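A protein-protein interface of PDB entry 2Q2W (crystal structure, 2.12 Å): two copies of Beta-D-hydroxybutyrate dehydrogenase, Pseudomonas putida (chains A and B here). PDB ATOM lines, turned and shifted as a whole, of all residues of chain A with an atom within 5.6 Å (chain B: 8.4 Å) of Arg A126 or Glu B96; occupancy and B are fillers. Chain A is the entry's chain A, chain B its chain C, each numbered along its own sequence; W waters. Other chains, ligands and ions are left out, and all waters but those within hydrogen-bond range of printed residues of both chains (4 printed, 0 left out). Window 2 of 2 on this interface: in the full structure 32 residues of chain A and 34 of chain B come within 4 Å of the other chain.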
ATOM      1  N   THR A 118      11.322 -21.529  13.258  1.00  0.00           N
ATOM      2  CA  THR A 118      10.989 -22.848  13.740  1.00  0.00           C
ATOM      3  C   THR A 118      11.663 -23.222  15.071  1.00  0.00           C
ATOM      4  O   THR A 118      11.022 -23.820  15.959  1.00  0.00           O
ATOM      5  CB  THR A 118      11.306 -23.948  12.658  1.00  0.00           C
ATOM      6  OG1 THR A 118      10.503 -23.732  11.506  1.00  0.00           O
ATOM      7  CG2 THR A 118      11.082 -25.264  13.199  1.00  0.00           C
ATOM      8  N   ARG A 119      12.947 -22.862  15.198  1.00  0.00           N
ATOM      9  CA  ARG A 119      13.703 -23.305  16.332  1.00  0.00           C
ATOM     10  C   ARG A 119      13.220 -22.512  17.564  1.00  0.00           C
ATOM     11  O   ARG A 119      13.190 -23.055  18.690  1.00  0.00           O
ATOM     12  CB  ARG A 119      15.212 -23.148  16.107  1.00  0.00           C
ATOM     13  CG  ARG A 119      15.768 -21.772  16.289  1.00  0.00           C
ATOM     14  CD  ARG A 119      17.171 -21.600  15.787  1.00  0.00           C
ATOM     15  NE  ARG A 119      17.517 -20.193  15.700  1.00  0.00           N
ATOM     16  CZ  ARG A 119      17.775 -19.388  16.737  1.00  0.00           C
ATOM     17  NH1 ARG A 119      17.793 -19.854  17.988  1.00  0.00           N
ATOM     18  NH2 ARG A 119      18.049 -18.101  16.508  1.00  0.00           N
ATOM     19  N   ALA A 121       9.998 -21.205  17.981  1.00  0.00           N
ATOM     20  CA  ALA A 121       8.572 -21.493  18.314  1.00  0.00           C
ATOM     21  C   ALA A 121       8.469 -22.915  18.885  1.00  0.00           C
ATOM     22  O   ALA A 121       7.574 -23.216  19.647  1.00  0.00           O
ATOM     23  CB  ALA A 121       7.712 -21.394  17.088  1.00  0.00           C
ATOM     24  N   LEU A 122       9.328 -23.822  18.446  1.00  0.00           N
ATOM     25  CA  LEU A 122       9.060 -25.242  18.711  1.00  0.00           C
ATOM     26  C   LEU A 122       9.193 -25.700  20.203  1.00  0.00           C
ATOM     27  O   LEU A 122       8.436 -26.574  20.637  1.00  0.00           O
ATOM     28  CB  LEU A 122       9.832 -26.162  17.762  1.00  0.00           C
ATOM     29  CG  LEU A 122       9.698 -27.674  17.911  1.00  0.00           C
ATOM     30  CD1 LEU A 122       8.211 -28.024  17.757  1.00  0.00           C
ATOM     31  CD2 LEU A 122      10.609 -28.438  16.840  1.00  0.00           C
ATOM     32  N   PRO A 123      10.152 -25.123  20.963  1.00  0.00           N
ATOM     33  CA  PRO A 123      10.146 -25.496  22.382  1.00  0.00           C
ATOM     34  C   PRO A 123       8.767 -25.190  23.087  1.00  0.00           C
ATOM     35  O   PRO A 123       8.345 -25.997  23.852  1.00  0.00           O
ATOM     36  CB  PRO A 123      11.312 -24.665  22.966  1.00  0.00           C
ATOM     37  CG  PRO A 123      12.220 -24.399  21.810  1.00  0.00           C
ATOM     38  CD  PRO A 123      11.274 -24.210  20.641  1.00  0.00           C
ATOM     39  N   GLY A 124       8.106 -24.042  22.830  1.00  0.00           N
ATOM     40  CA  GLY A 124       6.817 -23.676  23.521  1.00  0.00           C
ATOM     41  C   GLY A 124       5.694 -24.555  23.056  1.00  0.00           C
ATOM     42  O   GLY A 124       4.857 -24.987  23.867  1.00  0.00           O
ATOM     43  N   MET A 125       5.682 -24.858  21.740  1.00  0.00           N
ATOM     44  CA  MET A 125       4.702 -25.810  21.160  1.00  0.00           C
ATOM     45  C   MET A 125       4.853 -27.197  21.802  1.00  0.00           C
ATOM     46  O   MET A 125       3.824 -27.803  22.215  1.00  0.00           O
ATOM     47  CB  MET A 125       4.798 -25.901  19.663  1.00  0.00           C
ATOM     48  CG  MET A 125       4.458 -24.595  18.891  1.00  0.00           C
ATOM     49  SD  MET A 125       4.939 -24.699  17.121  1.00  0.00           S
ATOM     50  CE  MET A 125       4.256 -23.085  16.594  1.00  0.00           C
ATOM     51  N   ARG A 126       6.101 -27.683  21.943  1.00  0.00           N
ATOM     52  CA  ARG A 126       6.283 -29.004  22.642  1.00  0.00           C
ATOM     53  C   ARG A 126       5.851 -28.930  24.117  1.00  0.00           C
ATOM     54  O   ARG A 126       5.029 -29.745  24.512  1.00  0.00           O
ATOM     55  CB  ARG A 126       7.668 -29.694  22.493  1.00  0.00           C
ATOM     56  CG  ARG A 126       8.210 -29.897  21.084  1.00  0.00           C
ATOM     57  CD  ARG A 126       9.569 -30.513  21.223  1.00  0.00           C
ATOM     58  NE  ARG A 126      10.139 -31.042  19.975  1.00  0.00           N
ATOM     59  CZ  ARG A 126       9.811 -32.184  19.373  1.00  0.00           C
ATOM     60  NH1 ARG A 126       8.825 -32.958  19.846  1.00  0.00           N
ATOM     61  NH2 ARG A 126      10.471 -32.565  18.267  1.00  0.00           N
ATOM     62  N   ALA A 127       6.333 -27.924  24.893  1.00  0.00           N
ATOM     63  CA  ALA A 127       5.867 -27.730  26.271  1.00  0.00           C
ATOM     64  C   ALA A 127       4.315 -27.819  26.455  1.00  0.00           C
ATOM     65  O   ALA A 127       3.807 -28.428  27.416  1.00  0.00           O
ATOM     66  CB  ALA A 127       6.431 -26.374  26.873  1.00  0.00           C
ATOM     67  N   ARG A 128       3.573 -27.193  25.545  1.00  0.00           N
ATOM     68  CA  ARG A 128       2.128 -27.089  25.638  1.00  0.00           C
ATOM     69  C   ARG A 128       1.363 -28.249  24.948  1.00  0.00           C
ATOM     70  O   ARG A 128       0.091 -28.206  24.929  1.00  0.00           O
ATOM     71  CB  ARG A 128       1.661 -25.758  25.019  1.00  0.00           C
ATOM     72  CG  ARG A 128       2.080 -24.503  25.757  1.00  0.00           C
ATOM     73  CD  ARG A 128       1.862 -23.297  24.797  1.00  0.00           C
ATOM     74  NE  ARG A 128       3.010 -22.399  24.888  1.00  0.00           N
ATOM     75  CZ  ARG A 128       3.737 -21.934  23.882  1.00  0.00           C
ATOM     76  NH1 ARG A 128       3.466 -22.218  22.603  1.00  0.00           N
ATOM     77  NH2 ARG A 128       4.764 -21.140  24.196  1.00  0.00           N
ATOM     78  N   ASN A 129       2.123 -29.245  24.440  1.00  0.00           N
ATOM     79  CA  ASN A 129       1.744 -30.310  23.428  1.00  0.00           C
ATOM     80  C   ASN A 129       0.624 -29.954  22.472  1.00  0.00           C
ATOM     81  O   ASN A 129      -0.416 -30.615  22.456  1.00  0.00           O
ATOM     82  CB  ASN A 129       1.607 -31.804  23.993  1.00  0.00           C
ATOM     83  CG  ASN A 129       2.031 -32.944  22.917  1.00  0.00           C
ATOM     84  OD1 ASN A 129       2.592 -32.679  21.821  1.00  0.00           O
ATOM     85  ND2 ASN A 129       1.750 -34.219  23.280  1.00  0.00           N
ATOM     86  N   TRP A 130       0.881 -28.899  21.689  1.00  0.00           N
ATOM     87  CA  TRP A 130       0.019 -28.501  20.585  1.00  0.00           C
ATOM     88  C   TRP A 130       0.767 -27.499  19.757  1.00  0.00           C
ATOM     89  O   TRP A 130       1.255 -26.524  20.286  1.00  0.00           O
ATOM     90  CB  TRP A 130      -1.363 -27.908  21.046  1.00  0.00           C
ATOM     91  CG  TRP A 130      -2.315 -27.963  19.894  1.00  0.00           C
ATOM     92  CD1 TRP A 130      -3.064 -29.067  19.514  1.00  0.00           C
ATOM     93  CD2 TRP A 130      -2.478 -26.983  18.844  1.00  0.00           C
ATOM     94  NE1 TRP A 130      -3.726 -28.804  18.349  1.00  0.00           N
ATOM     95  CE2 TRP A 130      -3.393 -27.549  17.895  1.00  0.00           C
ATOM     96  CE3 TRP A 130      -1.952 -25.682  18.611  1.00  0.00           C
ATOM     97  CZ2 TRP A 130      -3.852 -26.843  16.749  1.00  0.00           C
ATOM     98  CZ3 TRP A 130      -2.419 -24.951  17.443  1.00  0.00           C
ATOM     99  CH2 TRP A 130      -3.334 -25.541  16.525  1.00  0.00           C
ATOM    100  N   GLU A 168      10.598 -34.909  13.071  1.00  0.00           N
ATOM    101  CA  GLU A 168      11.064 -34.727  14.404  1.00  0.00           C
ATOM    102  C   GLU A 168       9.924 -34.556  15.398  1.00  0.00           C
ATOM    103  O   GLU A 168      10.048 -34.884  16.595  1.00  0.00           O
ATOM    104  CB  GLU A 168      12.037 -33.535  14.488  1.00  0.00           C
ATOM    105  CG  GLU A 168      13.410 -33.883  13.876  1.00  0.00           C
ATOM    106  CD  GLU A 168      14.442 -32.762  14.062  1.00  0.00           C
ATOM    107  OE1 GLU A 168      14.167 -31.787  14.819  1.00  0.00           O
ATOM    108  OE2 GLU A 168      15.504 -32.870  13.433  1.00  0.00           O
ATOM    109  N   THR A 169       8.821 -34.080  14.860  1.00  0.00           N
ATOM    110  CA  THR A 169       7.632 -33.808  15.660  1.00  0.00           C
ATOM    111  C   THR A 169       6.578 -34.866  15.417  1.00  0.00           C
ATOM    112  O   THR A 169       5.466 -34.746  15.961  1.00  0.00           O
ATOM    113  CB  THR A 169       7.044 -32.357  15.386  1.00  0.00           C
ATOM    114  OG1 THR A 169       6.716 -32.164  13.994  1.00  0.00           O
ATOM    115  CG2 THR A 169       8.083 -31.231  15.805  1.00  0.00           C
ATOM    116  N   SER A 172       4.339 -36.188  18.338  1.00  0.00           N
ATOM    117  CA  SER A 172       3.820 -35.171  19.234  1.00  0.00           C
ATOM    118  C   SER A 172       2.520 -34.595  18.543  1.00  0.00           C
ATOM    119  O   SER A 172       2.207 -34.962  17.409  1.00  0.00           O
ATOM    120  CB  SER A 172       4.858 -34.042  19.381  1.00  0.00           C
ATOM    121  OG  SER A 172       4.755 -33.154  18.236  1.00  0.00           O
ATOM    122  N   VAL A 174       2.436 -31.501  17.653  1.00  0.00           N
ATOM    123  CA  VAL A 174       2.980 -30.472  16.838  1.00  0.00           C
ATOM    124  C   VAL A 174       3.144 -31.034  15.449  1.00  0.00           C
ATOM    125  O   VAL A 174       3.724 -32.104  15.299  1.00  0.00           O
ATOM    126  CB  VAL A 174       4.324 -29.924  17.414  1.00  0.00           C
ATOM    127  CG1 VAL A 174       4.829 -28.742  16.536  1.00  0.00           C
ATOM    128  CG2 VAL A 174       4.088 -29.492  18.973  1.00  0.00           C
ATOM    129  N   ALA B  93      21.569 -33.008  14.724  1.00  0.00           N
ATOM    130  CA  ALA B  93      20.901 -32.602  16.008  1.00  0.00           C
ATOM    131  C   ALA B  93      19.416 -32.177  15.756  1.00  0.00           C
ATOM    132  O   ALA B  93      19.101 -31.732  14.670  1.00  0.00           O
ATOM    133  CB  ALA B  93      21.715 -31.432  16.669  1.00  0.00           C
ATOM    134  N   PRO B  94      18.515 -32.348  16.744  1.00  0.00           N
ATOM    135  CA  PRO B  94      17.114 -31.896  16.607  1.00  0.00           C
ATOM    136  C   PRO B  94      17.061 -30.435  16.137  1.00  0.00           C
ATOM    137  O   PRO B  94      17.912 -29.671  16.534  1.00  0.00           O
ATOM    138  CB  PRO B  94      16.593 -31.967  18.067  1.00  0.00           C
ATOM    139  CG  PRO B  94      17.312 -33.195  18.654  1.00  0.00           C
ATOM    140  CD  PRO B  94      18.754 -32.949  18.109  1.00  0.00           C
ATOM    141  N   VAL B  95      16.078 -30.023  15.334  1.00  0.00           N
ATOM    142  CA  VAL B  95      16.137 -28.636  14.768  1.00  0.00           C
ATOM    143  C   VAL B  95      16.335 -27.516  15.856  1.00  0.00           C
ATOM    144  O   VAL B  95      17.104 -26.545  15.679  1.00  0.00           O
ATOM    145  CB  VAL B  95      14.904 -28.339  13.808  1.00  0.00           C
ATOM    146  CG1 VAL B  95      13.512 -28.270  14.663  1.00  0.00           C
ATOM    147  CG2 VAL B  95      15.128 -27.030  12.942  1.00  0.00           C
ATOM    148  N   GLU B  96      15.670 -27.690  17.017  1.00  0.00           N
ATOM    149  CA  GLU B  96      15.676 -26.691  18.124  1.00  0.00           C
ATOM    150  C   GLU B  96      16.890 -26.809  19.075  1.00  0.00           C
ATOM    151  O   GLU B  96      17.091 -25.945  19.897  1.00  0.00           O
ATOM    152  CB  GLU B  96      14.318 -26.622  18.887  1.00  0.00           C
ATOM    153  CG  GLU B  96      14.064 -27.733  19.972  1.00  0.00           C
ATOM    154  CD  GLU B  96      13.493 -29.032  19.392  1.00  0.00           C
ATOM    155  OE1 GLU B  96      12.488 -29.504  19.945  1.00  0.00           O
ATOM    156  OE2 GLU B  96      13.984 -29.573  18.361  1.00  0.00           O
ATOM    157  N   GLN B  97      17.730 -27.842  18.884  1.00  0.00           N
ATOM    158  CA  GLN B  97      19.033 -27.943  19.525  1.00  0.00           C
ATOM    159  C   GLN B  97      20.162 -27.828  18.501  1.00  0.00           C
ATOM    160  O   GLN B  97      21.274 -28.193  18.802  1.00  0.00           O
ATOM    161  CB  GLN B  97      19.166 -29.289  20.268  1.00  0.00           C
ATOM    162  CG  GLN B  97      17.938 -29.627  21.110  1.00  0.00           C
ATOM    163  CD  GLN B  97      18.189 -30.735  22.112  1.00  0.00           C
ATOM    164  OE1 GLN B  97      18.969 -31.704  21.884  1.00  0.00           O
ATOM    165  NE2 GLN B  97      17.516 -30.616  23.227  1.00  0.00           N
ATOM    166  N   PHE B  98      19.850 -27.395  17.277  1.00  0.00           N
ATOM    167  CA  PHE B  98      20.843 -27.276  16.220  1.00  0.00           C
ATOM    168  C   PHE B  98      21.747 -26.043  16.484  1.00  0.00           C
ATOM    169  O   PHE B  98      21.220 -24.951  16.604  1.00  0.00           O
ATOM    170  CB  PHE B  98      20.167 -27.185  14.865  1.00  0.00           C
ATOM    171  CG  PHE B  98      20.940 -27.797  13.759  1.00  0.00           C
ATOM    172  CD1 PHE B  98      20.745 -29.152  13.417  1.00  0.00           C
ATOM    173  CD2 PHE B  98      21.872 -27.036  13.022  1.00  0.00           C
ATOM    174  CE1 PHE B  98      21.468 -29.772  12.358  1.00  0.00           C
ATOM    175  CE2 PHE B  98      22.628 -27.677  11.960  1.00  0.00           C
ATOM    176  CZ  PHE B  98      22.390 -29.056  11.622  1.00  0.00           C
ATOM    177  N   PRO B  99      23.108 -26.222  16.530  1.00  0.00           N
ATOM    178  CA  PRO B  99      24.058 -25.112  16.641  1.00  0.00           C
ATOM    179  C   PRO B  99      23.851 -24.127  15.500  1.00  0.00           C
ATOM    180  O   PRO B  99      23.664 -24.520  14.329  1.00  0.00           O
ATOM    181  CB  PRO B  99      25.408 -25.817  16.487  1.00  0.00           C
ATOM    182  CG  PRO B  99      25.166 -27.159  16.927  1.00  0.00           C
ATOM    183  CD  PRO B  99      23.838 -27.497  16.405  1.00  0.00           C
ATOM    184  N   LEU B 100      23.820 -22.853  15.848  1.00  0.00           N
ATOM    185  CA  LEU B 100      23.487 -21.807  14.882  1.00  0.00           C
ATOM    186  C   LEU B 100      24.566 -21.684  13.792  1.00  0.00           C
ATOM    187  O   LEU B 100      24.261 -21.438  12.606  1.00  0.00           O
ATOM    188  CB  LEU B 100      23.279 -20.483  15.662  1.00  0.00           C
ATOM    189  CG  LEU B 100      21.829 -20.146  16.058  1.00  0.00           C
ATOM    190  CD1 LEU B 100      20.848 -21.281  16.324  1.00  0.00           C
ATOM    191  CD2 LEU B 100      21.668 -18.966  16.989  1.00  0.00           C
ATOM    192  N   THR B 146      15.299 -37.401  10.481  1.00  0.00           N
ATOM    193  CA  THR B 146      15.321 -36.680  11.735  1.00  0.00           C
ATOM    194  C   THR B 146      16.789 -36.298  12.051  1.00  0.00           C
ATOM    195  O   THR B 146      17.707 -37.046  11.685  1.00  0.00           O
ATOM    196  CB  THR B 146      14.841 -37.569  12.866  1.00  0.00           C
ATOM    197  OG1 THR B 146      15.629 -38.778  12.890  1.00  0.00           O
ATOM    198  CG2 THR B 146      13.368 -37.911  12.638  1.00  0.00           C
ATOM    199  N   ALA B 149      18.395 -31.162   9.802  1.00  0.00           N
ATOM    200  CA  ALA B 149      17.683 -29.967   9.289  1.00  0.00           C
ATOM    201  C   ALA B 149      18.508 -29.235   8.245  1.00  0.00           C
ATOM    202  O   ALA B 149      17.984 -28.926   7.171  1.00  0.00           O
ATOM    203  CB  ALA B 149      17.261 -28.992  10.419  1.00  0.00           C
HETATM  204  O   HOH W   1      12.867 -31.659  17.353  1.00  0.00           O
HETATM  205  O   HOH W   2      17.373 -31.190  12.755  1.00  0.00           O
HETATM  206  O   HOH W   3      17.540 -22.646  19.028  1.00  0.00           O
HETATM  207  O   HOH W   4      15.389 -22.925  20.355  1.00  0.00           O
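The guanidinium group (NE) of Arg A126 lies within salt-bridge range of the side-chain carboxylate (OE1) of Glu B96, 2.8 Å away.
OE1 of Glu A168 sits at hydrogen-bond distance from N of Val B95.
The backbone carbonyl oxygen (O) of Glu A168 is in hydrogen-bond range of the guanidinium group (NH2) of Arg A126 (2.9 Å).
Arg A119 touches Val B95.
Arg A119 touches Glu B96 (O to CB, 3.7 Å).
Leu B100 touches Arg A119 (CD1 to NE, 3.6 Å).
Leu A122 touches Val B95.
Leu A122 touches Glu B96 (CD2 to OE1, 3.8 Å).
O of Ala B93 touches OE2 of Glu A168, 3.97 Å away.
OE1 of Glu A168 touches CA of Pro B94, at 3.4 Å.
Thr B146 touches Glu A168.
Of the printed residues of chain B, Arg A126 touches Glu B96.
No residue of chain B comes within 4 Å of Ala A127.
Of the printed residues of chain A, Pro B94 touches Glu A168 (3.4 Å).
Printed residues of chain A within 4 Å of Val B95: Arg A119 (3.9 Å), Leu A122 (3.6 Å) and Glu A168 (2.7 Å).
Of chain A, only Arg A119 (3.7 Å), Leu A122 (3.8 Å) and Arg A126 (2.8 Å) come within 4 Å of Glu B96.
Of the 16 printed residues of chain A, 4 touch a printed residue of chain B.
Hydrophobic or aromatic side chains of chain A that line the printed part of chain B: Leu A122.
Along chain A the printed residues that touch a printed residue of chain B span positions 119 to 168.
Hydrophobic or aromatic side chains of chain B within 4 Å of the printed part of chain A: Val B95 and Leu B100.
Among the printed residues, Asp or Glu carboxylates within 4 Å of a Lys or Arg side-chain nitrogen of the other chain: Arg A126 with Glu B96 (2.8 Å).
No position is printed for both chains.
Of the 10 pairs that touch across the chains among the printed residues, none has its exchanged pair printed and touching as well.
Water W1 lies within hydrogen-bond range of the side-chain carboxylate of Glu B96 (2.6 Å), the guanidinium group of Arg A126 (2.7 Å) and the side-chain carboxylate of Glu A168 (2.9 Å).
Water W2 lies within hydrogen-bond range of the side-chain carboxylate of Glu A168 (2.6 Å), the backbone carbonyl oxygen of Ala B93 (2.6 Å), the backbone NH of Val B95 (3.1 Å) and the backbone NH of Ala B149 (3.1 Å).
Water W4 bridges O of Arg A119 (2.8 Å) and O of Glu B96 (3.5 Å).
Water W3 bridges the guanidinium group (NH1) of Arg A119 (3.0 Å) and the backbone carbonyl oxygen (O) of Glu B96 (3.4 Å).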
